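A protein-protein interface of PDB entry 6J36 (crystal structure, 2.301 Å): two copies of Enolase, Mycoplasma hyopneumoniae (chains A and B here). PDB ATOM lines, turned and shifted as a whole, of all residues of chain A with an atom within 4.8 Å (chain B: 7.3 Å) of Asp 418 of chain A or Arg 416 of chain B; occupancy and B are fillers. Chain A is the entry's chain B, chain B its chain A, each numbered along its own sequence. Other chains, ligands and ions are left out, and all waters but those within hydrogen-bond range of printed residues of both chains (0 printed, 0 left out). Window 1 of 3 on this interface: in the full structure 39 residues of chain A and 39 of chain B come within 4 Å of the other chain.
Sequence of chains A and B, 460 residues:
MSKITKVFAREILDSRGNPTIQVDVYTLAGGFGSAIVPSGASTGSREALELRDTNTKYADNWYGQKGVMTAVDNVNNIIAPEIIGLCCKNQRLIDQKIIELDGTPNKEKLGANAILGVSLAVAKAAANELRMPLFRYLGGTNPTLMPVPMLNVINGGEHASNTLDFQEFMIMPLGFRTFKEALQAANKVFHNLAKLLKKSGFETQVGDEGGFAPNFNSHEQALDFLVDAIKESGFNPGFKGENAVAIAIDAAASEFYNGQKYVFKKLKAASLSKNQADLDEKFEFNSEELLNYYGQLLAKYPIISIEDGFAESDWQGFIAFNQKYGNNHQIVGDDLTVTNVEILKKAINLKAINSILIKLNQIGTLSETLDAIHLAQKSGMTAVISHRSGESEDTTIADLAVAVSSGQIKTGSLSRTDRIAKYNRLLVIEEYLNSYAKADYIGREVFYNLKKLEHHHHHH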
ATOM      1  N   SER A  15      32.788  -4.569  22.597  1.00  0.00           N
ATOM      2  CA  SER A  15      32.370  -3.403  23.374  1.00  0.00           C
ATOM      3  C   SER A  15      33.011  -2.102  22.902  1.00  0.00           C
ATOM      4  O   SER A  15      32.631  -1.032  23.388  1.00  0.00           O
ATOM      5  CB  SER A  15      32.675  -3.615  24.855  1.00  0.00           C
ATOM      6  OG  SER A  15      34.067  -3.744  25.081  1.00  0.00           O
ATOM      7  N   VAL A 206      34.202   8.045  30.755  1.00  0.00           N
ATOM      8  CA  VAL A 206      34.974   6.827  30.986  1.00  0.00           C
ATOM      9  C   VAL A 206      35.628   6.336  29.694  1.00  0.00           C
ATOM     10  O   VAL A 206      35.212   6.672  28.583  1.00  0.00           O
ATOM     11  CB  VAL A 206      34.107   5.712  31.610  1.00  0.00           C
ATOM     12  CG1 VAL A 206      33.412   6.237  32.861  1.00  0.00           C
ATOM     13  CG2 VAL A 206      33.085   5.193  30.597  1.00  0.00           C
ATOM     14  N   ASP A 208      37.737   2.629  27.909  1.00  0.00           N
ATOM     15  CA  ASP A 208      37.370   1.283  27.464  1.00  0.00           C
ATOM     16  C   ASP A 208      37.038   0.341  28.621  1.00  0.00           C
ATOM     17  O   ASP A 208      36.268  -0.608  28.432  1.00  0.00           O
ATOM     18  CB  ASP A 208      38.503   0.680  26.626  1.00  0.00           C
ATOM     19  CG  ASP A 208      38.619   1.314  25.237  1.00  0.00           C
ATOM     20  OD1 ASP A 208      37.589   1.795  24.711  1.00  0.00           O
ATOM     21  OD2 ASP A 208      39.736   1.316  24.661  1.00  0.00           O
ATOM     22  N   GLU A 391      35.619  -6.232  24.798  1.00  0.00           N
ATOM     23  CA  GLU A 391      34.993  -7.296  25.577  1.00  0.00           C
ATOM     24  C   GLU A 391      33.519  -7.460  25.230  1.00  0.00           C
ATOM     25  O   GLU A 391      33.017  -6.854  24.277  1.00  0.00           O
ATOM     26  CB  GLU A 391      35.142  -7.023  27.074  1.00  0.00           C
ATOM     27  CG  GLU A 391      36.439  -7.508  27.666  1.00  0.00           C
ATOM     28  CD  GLU A 391      36.461  -9.015  27.930  1.00  0.00           C
ATOM     29  OE1 GLU A 391      37.561  -9.568  28.144  1.00  0.00           O
ATOM     30  OE2 GLU A 391      35.389  -9.654  27.929  1.00  0.00           O
ATOM     31  N   SER A 392      32.820  -8.276  26.004  1.00  0.00           N
ATOM     32  CA  SER A 392      31.426  -8.574  25.723  1.00  0.00           C
ATOM     33  C   SER A 392      30.784  -9.044  27.019  1.00  0.00           C
ATOM     34  O   SER A 392      31.406  -9.004  28.088  1.00  0.00           O
ATOM     35  CB  SER A 392      31.315  -9.625  24.614  1.00  0.00           C
ATOM     36  OG  SER A 392      31.552 -10.904  25.163  1.00  0.00           O
ATOM     37  N   SER A 415      31.670   0.361  35.724  1.00  0.00           N
ATOM     38  CA  SER A 415      30.643   0.753  34.760  1.00  0.00           C
ATOM     39  C   SER A 415      30.922   0.028  33.458  1.00  0.00           C
ATOM     40  O   SER A 415      31.995  -0.546  33.281  1.00  0.00           O
ATOM     41  CB  SER A 415      30.583   2.273  34.551  1.00  0.00           C
ATOM     42  OG  SER A 415      31.728   2.764  33.889  1.00  0.00           O
ATOM     43  N   ARG A 416      29.935   0.065  32.552  1.00  0.00           N
ATOM     44  CA  ARG A 416      29.881  -0.686  31.293  1.00  0.00           C
ATOM     45  C   ARG A 416      29.571  -2.157  31.540  1.00  0.00           C
ATOM     46  O   ARG A 416      30.243  -2.815  32.343  1.00  0.00           O
ATOM     47  CB  ARG A 416      31.188  -0.585  30.491  1.00  0.00           C
ATOM     48  CG  ARG A 416      31.647   0.821  30.157  1.00  0.00           C
ATOM     49  CD  ARG A 416      33.056   0.773  29.574  1.00  0.00           C
ATOM     50  NE  ARG A 416      33.080   0.157  28.256  1.00  0.00           N
ATOM     51  CZ  ARG A 416      33.312   0.816  27.131  1.00  0.00           C
ATOM     52  NH1 ARG A 416      33.546   2.124  27.164  1.00  0.00           N
ATOM     53  NH2 ARG A 416      33.317   0.170  25.977  1.00  0.00           N
ATOM     54  N   THR A 417      28.580  -2.691  30.822  1.00  0.00           N
ATOM     55  CA  THR A 417      28.246  -4.103  30.972  1.00  0.00           C
ATOM     56  C   THR A 417      29.414  -5.022  30.596  1.00  0.00           C
ATOM     57  O   THR A 417      29.508  -6.133  31.129  1.00  0.00           O
ATOM     58  CB  THR A 417      27.000  -4.425  30.146  1.00  0.00           C
ATOM     59  OG1 THR A 417      25.889  -3.671  30.652  1.00  0.00           O
ATOM     60  CG2 THR A 417      26.661  -5.906  30.207  1.00  0.00           C
ATOM     61  N   ASP A 418      30.313  -4.591  29.693  1.00  0.00           N
ATOM     62  CA  ASP A 418      31.453  -5.445  29.323  1.00  0.00           C
ATOM     63  C   ASP A 418      32.350  -5.782  30.508  1.00  0.00           C
ATOM     64  O   ASP A 418      33.033  -6.807  30.478  1.00  0.00           O
ATOM     65  CB  ASP A 418      32.284  -4.817  28.198  1.00  0.00           C
ATOM     66  CG  ASP A 418      32.528  -3.323  28.399  1.00  0.00           C
ATOM     67  OD1 ASP A 418      31.542  -2.556  28.322  1.00  0.00           O
ATOM     68  OD2 ASP A 418      33.690  -2.916  28.603  1.00  0.00           O
ATOM     69  N   ARG A 419      32.343  -4.967  31.560  1.00  0.00           N
ATOM     70  CA  ARG A 419      32.967  -5.300  32.833  1.00  0.00           C
ATOM     71  C   ARG A 419      31.960  -5.775  33.878  1.00  0.00           C
ATOM     72  O   ARG A 419      32.209  -6.766  34.577  1.00  0.00           O
ATOM     73  CB  ARG A 419      33.723  -4.077  33.375  1.00  0.00           C
ATOM     74  CG  ARG A 419      34.413  -3.197  32.317  1.00  0.00           C
ATOM     75  CD  ARG A 419      35.514  -3.945  31.555  1.00  0.00           C
ATOM     76  NE  ARG A 419      35.360  -3.692  30.128  1.00  0.00           N
ATOM     77  CZ  ARG A 419      36.253  -3.968  29.182  1.00  0.00           C
ATOM     78  NH1 ARG A 419      37.410  -4.521  29.490  1.00  0.00           N
ATOM     79  NH2 ARG A 419      35.975  -3.700  27.913  1.00  0.00           N
ATOM     80  N   ILE A 420      30.816  -5.092  33.979  1.00  0.00           N
ATOM     81  CA  ILE A 420      29.867  -5.333  35.062  1.00  0.00           C
ATOM     82  C   ILE A 420      29.380  -6.778  35.045  1.00  0.00           C
ATOM     83  O   ILE A 420      29.252  -7.415  36.097  1.00  0.00           O
ATOM     84  CB  ILE A 420      28.703  -4.325  34.961  1.00  0.00           C
ATOM     85  CG1 ILE A 420      29.155  -2.912  35.409  1.00  0.00           C
ATOM     86  CG2 ILE A 420      27.455  -4.837  35.714  1.00  0.00           C
ATOM     87  CD1 ILE A 420      29.294  -2.739  36.889  1.00  0.00           C
ATOM     88  N   LYS A 422      30.894  -9.448  34.471  1.00  0.00           N
ATOM     89  CA  LYS A 422      31.765 -10.370  35.190  1.00  0.00           C
ATOM     90  C   LYS A 422      31.524 -10.274  36.694  1.00  0.00           C
ATOM     91  O   LYS A 422      31.483 -11.297  37.386  1.00  0.00           O
ATOM     92  CB  LYS A 422      33.232 -10.118  34.841  1.00  0.00           C
ATOM     93  CG  LYS A 422      33.683 -10.682  33.478  1.00  0.00           C
ATOM     94  CD  LYS A 422      33.223  -9.835  32.303  1.00  0.00           C
ATOM     95  CE  LYS A 422      34.125 -10.054  31.111  1.00  0.00           C
ATOM     96  NZ  LYS A 422      33.503  -9.653  29.812  1.00  0.00           N
ATOM     97  N   ASP B  14      23.884  -2.707  37.384  1.00  0.00           N
ATOM     98  CA  ASP B  14      23.604  -2.226  36.040  1.00  0.00           C
ATOM     99  C   ASP B  14      24.863  -1.580  35.447  1.00  0.00           C
ATOM    100  O   ASP B  14      25.930  -1.541  36.069  1.00  0.00           O
ATOM    101  CB  ASP B  14      22.370  -1.291  36.047  1.00  0.00           C
ATOM    102  CG  ASP B  14      22.656   0.147  36.574  1.00  0.00           C
ATOM    103  OD1 ASP B  14      23.825   0.550  36.791  1.00  0.00           O
ATOM    104  OD2 ASP B  14      21.672   0.902  36.751  1.00  0.00           O
ATOM    105  N   SER B  15      24.737  -1.066  34.224  1.00  0.00           N
ATOM    106  CA  SER B  15      25.914  -0.620  33.488  1.00  0.00           C
ATOM    107  C   SER B  15      26.479   0.691  34.010  1.00  0.00           C
ATOM    108  O   SER B  15      27.539   1.117  33.550  1.00  0.00           O
ATOM    109  CB  SER B  15      25.588  -0.474  32.007  1.00  0.00           C
ATOM    110  OG  SER B  15      24.604   0.525  31.823  1.00  0.00           O
ATOM    111  N   ARG B  16      25.802   1.340  34.952  1.00  0.00           N
ATOM    112  CA  ARG B  16      26.350   2.498  35.632  1.00  0.00           C
ATOM    113  C   ARG B  16      26.879   2.139  37.010  1.00  0.00           C
ATOM    114  O   ARG B  16      27.230   3.032  37.781  1.00  0.00           O
ATOM    115  CB  ARG B  16      25.291   3.582  35.758  1.00  0.00           C
ATOM    116  CG  ARG B  16      24.816   4.129  34.453  1.00  0.00           C
ATOM    117  CD  ARG B  16      24.276   5.508  34.698  1.00  0.00           C
ATOM    118  NE  ARG B  16      22.837   5.496  34.852  1.00  0.00           N
ATOM    119  CZ  ARG B  16      22.165   6.331  35.634  1.00  0.00           C
ATOM    120  NH1 ARG B  16      22.813   7.236  36.362  1.00  0.00           N
ATOM    121  NH2 ARG B  16      20.842   6.246  35.694  1.00  0.00           N
ATOM    122  N   GLY B  17      26.908   0.855  37.349  1.00  0.00           N
ATOM    123  CA  GLY B  17      27.374   0.470  38.663  1.00  0.00           C
ATOM    124  C   GLY B  17      26.387   0.685  39.785  1.00  0.00           C
ATOM    125  O   GLY B  17      26.803   0.856  40.934  1.00  0.00           O
ATOM    126  N   PHE B 190      30.963   6.207  13.158  1.00  0.00           N
ATOM    127  CA  PHE B 190      31.340   6.296  14.569  1.00  0.00           C
ATOM    128  C   PHE B 190      32.854   6.383  14.742  1.00  0.00           C
ATOM    129  O   PHE B 190      33.363   7.246  15.465  1.00  0.00           O
ATOM    130  CB  PHE B 190      30.769   5.077  15.319  1.00  0.00           C
ATOM    131  CG  PHE B 190      31.227   4.940  16.770  1.00  0.00           C
ATOM    132  CD1 PHE B 190      30.582   5.639  17.793  1.00  0.00           C
ATOM    133  CD2 PHE B 190      32.274   4.078  17.112  1.00  0.00           C
ATOM    134  CE1 PHE B 190      30.982   5.498  19.142  1.00  0.00           C
ATOM    135  CE2 PHE B 190      32.681   3.933  18.454  1.00  0.00           C
ATOM    136  CZ  PHE B 190      32.025   4.645  19.472  1.00  0.00           C
ATOM    137  N   VAL B 206      33.708   8.336  26.739  1.00  0.00           N
ATOM    138  CA  VAL B 206      32.291   8.173  26.450  1.00  0.00           C
ATOM    139  C   VAL B 206      31.480   8.324  27.739  1.00  0.00           C
ATOM    140  O   VAL B 206      32.009   8.239  28.852  1.00  0.00           O
ATOM    141  CB  VAL B 206      31.993   6.818  25.766  1.00  0.00           C
ATOM    142  CG1 VAL B 206      32.788   6.693  24.471  1.00  0.00           C
ATOM    143  CG2 VAL B 206      32.306   5.672  26.706  1.00  0.00           C
ATOM    144  N   GLY B 207      30.184   8.581  27.562  1.00  0.00           N
ATOM    145  CA  GLY B 207      29.233   8.656  28.647  1.00  0.00           C
ATOM    146  C   GLY B 207      28.400   7.390  28.787  1.00  0.00           C
ATOM    147  O   GLY B 207      28.769   6.299  28.327  1.00  0.00           O
ATOM    148  N   ASP B 208      27.240   7.551  29.416  1.00  0.00           N
ATOM    149  CA  ASP B 208      26.399   6.418  29.781  1.00  0.00           C
ATOM    150  C   ASP B 208      25.993   5.577  28.580  1.00  0.00           C
ATOM    151  O   ASP B 208      25.864   4.353  28.707  1.00  0.00           O
ATOM    152  CB  ASP B 208      25.157   6.923  30.513  1.00  0.00           C
ATOM    153  CG  ASP B 208      25.460   7.368  31.930  1.00  0.00           C
ATOM    154  OD1 ASP B 208      26.523   6.984  32.461  1.00  0.00           O
ATOM    155  OD2 ASP B 208      24.649   8.116  32.506  1.00  0.00           O
ATOM    156  N   GLU B 209      25.778   6.196  27.414  1.00  0.00           N
ATOM    157  CA  GLU B 209      25.301   5.466  26.242  1.00  0.00           C
ATOM    158  C   GLU B 209      26.405   5.144  25.250  1.00  0.00           C
ATOM    159  O   GLU B 209      26.106   4.673  24.143  1.00  0.00           O
ATOM    160  CB  GLU B 209      24.193   6.241  25.521  1.00  0.00           C
ATOM    161  CG  GLU B 209      23.158   6.816  26.432  1.00  0.00           C
ATOM    162  CD  GLU B 209      23.383   8.301  26.700  1.00  0.00           C
ATOM    163  OE1 GLU B 209      24.525   8.694  27.078  1.00  0.00           O
ATOM    164  OE2 GLU B 209      22.408   9.073  26.529  1.00  0.00           O
ATOM    165  N   GLY B 210      27.660   5.383  25.615  1.00  0.00           N
ATOM    166  CA  GLY B 210      28.784   5.060  24.765  1.00  0.00           C
ATOM    167  C   GLY B 210      29.054   6.023  23.632  1.00  0.00           C
ATOM    168  O   GLY B 210      29.796   5.663  22.708  1.00  0.00           O
ATOM    169  N   GLY B 211      28.448   7.212  23.651  1.00  0.00           N
ATOM    170  CA  GLY B 211      28.774   8.272  22.725  1.00  0.00           C
ATOM    171  C   GLY B 211      29.681   9.335  23.345  1.00  0.00           C
ATOM    172  O   GLY B 211      30.092   9.258  24.501  1.00  0.00           O
ATOM    173  N   SER B 389      19.246   4.859  30.573  1.00  0.00           N
ATOM    174  CA  SER B 389      20.629   5.199  30.891  1.00  0.00           C
ATOM    175  C   SER B 389      21.344   4.045  31.587  1.00  0.00           C
ATOM    176  O   SER B 389      22.524   3.789  31.319  1.00  0.00           O
ATOM    177  CB  SER B 389      20.675   6.450  31.765  1.00  0.00           C
ATOM    178  OG  SER B 389      20.275   7.592  31.027  1.00  0.00           O
ATOM    179  N   GLY B 390      20.660   3.366  32.507  1.00  0.00           N
ATOM    180  CA  GLY B 390      21.212   2.218  33.199  1.00  0.00           C
ATOM    181  C   GLY B 390      20.690   0.949  32.567  1.00  0.00           C
ATOM    182  O   GLY B 390      19.483   0.736  32.493  1.00  0.00           O
ATOM    183  N   GLU B 391      21.607   0.108  32.087  1.00  0.00           N
ATOM    184  CA  GLU B 391      21.264  -0.972  31.173  1.00  0.00           C
ATOM    185  C   GLU B 391      22.081  -2.211  31.515  1.00  0.00           C
ATOM    186  O   GLU B 391      22.883  -2.210  32.449  1.00  0.00           O
ATOM    187  CB  GLU B 391      21.508  -0.567  29.708  1.00  0.00           C
ATOM    188  CG  GLU B 391      20.362   0.148  29.066  1.00  0.00           C
ATOM    189  CD  GLU B 391      19.199  -0.783  28.758  1.00  0.00           C
ATOM    190  OE1 GLU B 391      18.097  -0.273  28.449  1.00  0.00           O
ATOM    191  OE2 GLU B 391      19.394  -2.022  28.815  1.00  0.00           O
ATOM    192  N   THR B 411      18.953   2.746  21.040  1.00  0.00           N
ATOM    193  CA  THR B 411      19.601   1.931  22.055  1.00  0.00           C
ATOM    194  C   THR B 411      21.092   2.245  22.167  1.00  0.00           C
ATOM    195  O   THR B 411      21.880   1.406  22.632  1.00  0.00           O
ATOM    196  CB  THR B 411      19.346   0.436  21.796  1.00  0.00           C
ATOM    197  OG1 THR B 411      19.797  -0.329  22.922  1.00  0.00           O
ATOM    198  CG2 THR B 411      20.037  -0.058  20.509  1.00  0.00           C
ATOM    199  N   SER B 413      24.988   4.469  21.504  1.00  0.00           N
ATOM    200  CA  SER B 413      26.066   4.595  20.535  1.00  0.00           C
ATOM    201  C   SER B 413      26.616   3.216  20.182  1.00  0.00           C
ATOM    202  O   SER B 413      26.022   2.190  20.516  1.00  0.00           O
ATOM    203  CB  SER B 413      27.148   5.512  21.078  1.00  0.00           C
ATOM    204  OG  SER B 413      27.800   6.141  19.996  1.00  0.00           O
ATOM    205  N   LEU B 414      27.762   3.176  19.501  1.00  0.00           N
ATOM    206  CA  LEU B 414      28.410   1.908  19.145  1.00  0.00           C
ATOM    207  C   LEU B 414      29.611   1.601  20.039  1.00  0.00           C
ATOM    208  O   LEU B 414      30.678   1.198  19.563  1.00  0.00           O
ATOM    209  CB  LEU B 414      28.826   1.923  17.685  1.00  0.00           C
ATOM    210  CG  LEU B 414      27.856   1.444  16.609  1.00  0.00           C
ATOM    211  CD1 LEU B 414      28.668   1.045  15.422  1.00  0.00           C
ATOM    212  CD2 LEU B 414      27.015   0.275  17.022  1.00  0.00           C
ATOM    213  N   SER B 415      29.460   1.783  21.345  1.00  0.00           N
ATOM    214  CA  SER B 415      30.396   1.194  22.290  1.00  0.00           C
ATOM    215  C   SER B 415      29.635   0.895  23.569  1.00  0.00           C
ATOM    216  O   SER B 415      28.528   1.394  23.774  1.00  0.00           O
ATOM    217  CB  SER B 415      31.613   2.096  22.538  1.00  0.00           C
ATOM    218  OG  SER B 415      31.267   3.285  23.221  1.00  0.00           O
ATOM    219  N   ARG B 416      30.247   0.065  24.416  1.00  0.00           N
ATOM    220  CA  ARG B 416      29.685  -0.492  25.650  1.00  0.00           C
ATOM    221  C   ARG B 416      28.729  -1.630  25.333  1.00  0.00           C
ATOM    222  O   ARG B 416      27.792  -1.475  24.532  1.00  0.00           O
ATOM    223  CB  ARG B 416      28.948   0.545  26.515  1.00  0.00           C
ATOM    224  CG  ARG B 416      29.780   1.740  26.927  1.00  0.00           C
ATOM    225  CD  ARG B 416      28.886   2.816  27.546  1.00  0.00           C
ATOM    226  NE  ARG B 416      28.377   2.403  28.850  1.00  0.00           N
ATOM    227  CZ  ARG B 416      28.697   2.977  30.007  1.00  0.00           C
ATOM    228  NH1 ARG B 416      29.523   4.016  30.036  1.00  0.00           N
ATOM    229  NH2 ARG B 416      28.181   2.515  31.136  1.00  0.00           N
ATOM    230  N   THR B 417      28.947  -2.769  25.992  1.00  0.00           N
ATOM    231  CA  THR B 417      28.081  -3.919  25.777  1.00  0.00           C
ATOM    232  C   THR B 417      26.626  -3.597  26.102  1.00  0.00           C
ATOM    233  O   THR B 417      25.726  -4.183  25.493  1.00  0.00           O
ATOM    234  CB  THR B 417      28.596  -5.100  26.602  1.00  0.00           C
ATOM    235  OG1 THR B 417      29.917  -5.406  26.164  1.00  0.00           O
ATOM    236  CG2 THR B 417      27.724  -6.351  26.448  1.00  0.00           C
ATOM    237  N   ASP B 418      26.370  -2.649  27.025  1.00  0.00           N
ATOM    238  CA  ASP B 418      24.987  -2.322  27.376  1.00  0.00           C
ATOM    239  C   ASP B 418      24.204  -1.782  26.187  1.00  0.00           C
ATOM    240  O   ASP B 418      22.974  -1.878  26.168  1.00  0.00           O
ATOM    241  CB  ASP B 418      24.896  -1.337  28.564  1.00  0.00           C
ATOM    242  CG  ASP B 418      25.845  -0.138  28.451  1.00  0.00           C
ATOM    243  OD1 ASP B 418      27.090  -0.347  28.425  1.00  0.00           O
ATOM    244  OD2 ASP B 418      25.339   1.016  28.440  1.00  0.00           O
ATOM    245  N   ARG B 419      24.885  -1.243  25.190  1.00  0.00           N
ATOM    246  CA  ARG B 419      24.273  -0.865  23.928  1.00  0.00           C
ATOM    247  C   ARG B 419      24.545  -1.887  22.823  1.00  0.00           C
ATOM    248  O   ARG B 419      23.621  -2.266  22.095  1.00  0.00           O
ATOM    249  CB  ARG B 419      24.790   0.521  23.508  1.00  0.00           C
ATOM    250  CG  ARG B 419      25.047   1.492  24.668  1.00  0.00           C
ATOM    251  CD  ARG B 419      23.761   1.879  25.436  1.00  0.00           C
ATOM    252  NE  ARG B 419      23.984   1.835  26.878  1.00  0.00           N
ATOM    253  CZ  ARG B 419      23.098   2.199  27.806  1.00  0.00           C
ATOM    254  NH1 ARG B 419      21.906   2.659  27.455  1.00  0.00           N
ATOM    255  NH2 ARG B 419      23.416   2.113  29.093  1.00  0.00           N
ATOM    256  N   ILE B 420      25.789  -2.378  22.731  1.00  0.00           N
ATOM    257  CA  ILE B 420      26.232  -3.231  21.622  1.00  0.00           C
ATOM    258  C   ILE B 420      25.445  -4.540  21.585  1.00  0.00           C
ATOM    259  O   ILE B 420      25.104  -5.047  20.507  1.00  0.00           O
ATOM    260  CB  ILE B 420      27.754  -3.471  21.740  1.00  0.00           C
ATOM    261  CG1 ILE B 420      28.533  -2.239  21.273  1.00  0.00           C
ATOM    262  CG2 ILE B 420      28.205  -4.701  20.981  1.00  0.00           C
ATOM    263  CD1 ILE B 420      28.342  -1.955  19.828  1.00  0.00           C
ATOM    264  N   ALA B 421      25.120  -5.094  22.758  1.00  0.00           N
ATOM    265  CA  ALA B 421      24.366  -6.347  22.800  1.00  0.00           C
ATOM    266  C   ALA B 421      23.050  -6.251  22.028  1.00  0.00           C
ATOM    267  O   ALA B 421      22.602  -7.243  21.443  1.00  0.00           O
ATOM    268  CB  ALA B 421      24.093  -6.765  24.256  1.00  0.00           C
ATOM    269  N   LYS B 422      22.404  -5.084  22.026  1.00  0.00           N
ATOM    270  CA  LYS B 422      21.142  -4.959  21.306  1.00  0.00           C
ATOM    271  C   LYS B 422      21.366  -4.999  19.799  1.00  0.00           C
ATOM    272  O   LYS B 422      20.570  -5.594  19.065  1.00  0.00           O
ATOM    273  CB  LYS B 422      20.426  -3.665  21.701  1.00  0.00           C
ATOM    274  CG  LYS B 422      19.626  -3.728  23.023  1.00  0.00           C
ATOM    275  CD  LYS B 422      20.538  -3.700  24.245  1.00  0.00           C
ATOM    276  CE  LYS B 422      19.837  -3.037  25.446  1.00  0.00           C
ATOM    277  NZ  LYS B 422      20.601  -3.195  26.713  1.00  0.00           N
ATOM    278  N   TYR B 423      22.431  -4.354  19.312  1.00  0.00           N
ATOM    279  CA  TYR B 423      22.719  -4.435  17.883  1.00  0.00           C
ATOM    280  C   TYR B 423      23.106  -5.854  17.504  1.00  0.00           C
ATOM    281  O   TYR B 423      22.733  -6.340  16.429  1.00  0.00           O
ATOM    282  CB  TYR B 423      23.824  -3.449  17.493  1.00  0.00           C
ATOM    283  CG  TYR B 423      23.462  -2.013  17.787  1.00  0.00           C
ATOM    284  CD1 TYR B 423      22.402  -1.406  17.133  1.00  0.00           C
ATOM    285  CD2 TYR B 423      24.181  -1.260  18.715  1.00  0.00           C
ATOM    286  CE1 TYR B 423      22.058  -0.088  17.391  1.00  0.00           C
ATOM    287  CE2 TYR B 423      23.841   0.064  18.989  1.00  0.00           C
ATOM    288  CZ  TYR B 423      22.774   0.634  18.325  1.00  0.00           C
ATOM    289  OH  TYR B 423      22.421   1.932  18.579  1.00  0.00           O
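Of the 26 printed residues of chain B, 8 touch a printed residue of chain A. Of the 12 printed residues of chain A, 9 touch a printed residue of chain B. Hydrophobic or aromatic side chains of chain A within 4 Å of the printed part of chain B: Val 206 and Ile 420.
Ser 415 of chain B touches Ser 15 of chain A. Arg 416 of chain B touches Val 206 of chain A. Thr 417 of chain B touches Glu 391 of chain A (OG1 to O, 3.9 Å). CA of Ser 392 of chain A touches OG1 of Thr 417 of chain B (3.5 Å). CA of Ser 415 of chain A touches O of Ser 15 of chain B, 3.4 Å away. Ser 15 of chain B touches Thr 417 of chain A. Thr 417 of chain A touches Glu 391 of chain B (OG1 to O, 3.8 Å). Asp 418 of chain B touches Thr 417 of chain A. OD1 of Asp 418 of chain A touches CA of Arg 416 of chain B, 3.9 Å away. Ile 420 of chain A touches Asp 14 of chain B.
Arg 416 of chain B touches just these residues of chain A: Ser 15, Val 206, Arg 416 and Asp 418. Of the printed residues of chain B, Ile 420 of chain A touches Asp 14 (3.6 Å). Of the printed residues of chain B, Thr 417 of chain A touches Ser 15 (3.5 Å), Glu 391 (3.8 Å), Thr 417 (3.9 Å) and Asp 418 (3.3 Å). Of the printed residues of chain A, Asp 14 of chain B touches Ile 420. Of the printed residues of chain B, Ser 15 of chain A touches Ser 415, Arg 416 and Thr 417.
The backbone carbonyl oxygen (O) of Ser 15 of chain A lies within hydrogen-bond range of the backbone NH (N) of Arg 416 of chain B (2.8 Å). The backbone NH (N) of Thr 417 of chain B lies within hydrogen-bond range of the side-chain carboxylate (OD1) of Asp 418 of chain A (3.5 Å). The backbone carbonyl oxygen (O) of Ser 15 of chain B is in hydrogen-bond range of the backbone NH (N) of Arg 416 of chain A (2.8 Å). N of Arg 416 of chain A sits close to NH2 of Arg 416 of chain B. The backbone NH of Val 206 of chain B lies within hydrogen-bond range of the backbone carbonyl oxygen of Val 206 of chain A (2.9 Å).
The side-chain carboxylate (OD1) of Asp 418 of chain B is in salt-bridge range of the guanidinium group (NE) of Arg 416 of chain B, 3.1 Å away. O of Asp 208 of chain A lies within hydrogen-bond range of NE of Arg 416 of chain A (3.3 Å). The side-chain carboxylate of Asp 418 of chain B lies within hydrogen-bond range of the side-chain hydroxyl of Ser 15 of chain B. The guanidinium group (NH2) of Arg 419 of chain B lies within hydrogen-bond range of the side-chain hydroxyl (OG) of Ser 15 of chain B, 3.4 Å away. OD1 of Asp 418 of chain A is in salt-bridge range of NE of Arg 416 of chain A (3.1 Å). The backbone carbonyl oxygen (O) of Gly 207 of chain B sits at hydrogen-bond distance from the guanidinium group (NH1) of Arg 416 of chain B, 2.9 Å away.
Ser 15 of chain A touches Arg 416 of chain B, and with the chains exchanged Arg 416 of chain A touches Ser 15 of chain B. Ser 15 of chain A touches Thr 417 of chain B, and with the chains exchanged Thr 417 of chain A touches Ser 15 of chain B. Glu 391 of chain A touches Thr 417 of chain B, and with the chains exchanged Thr 417 of chain A touches Glu 391 of chain B. Thr 417 of chain B touches its own counterpart, Thr 417 of chain A. Of the 18 pairs that touch across the chains among the printed residues, 15 have their exchanged pair printed and touching as well.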
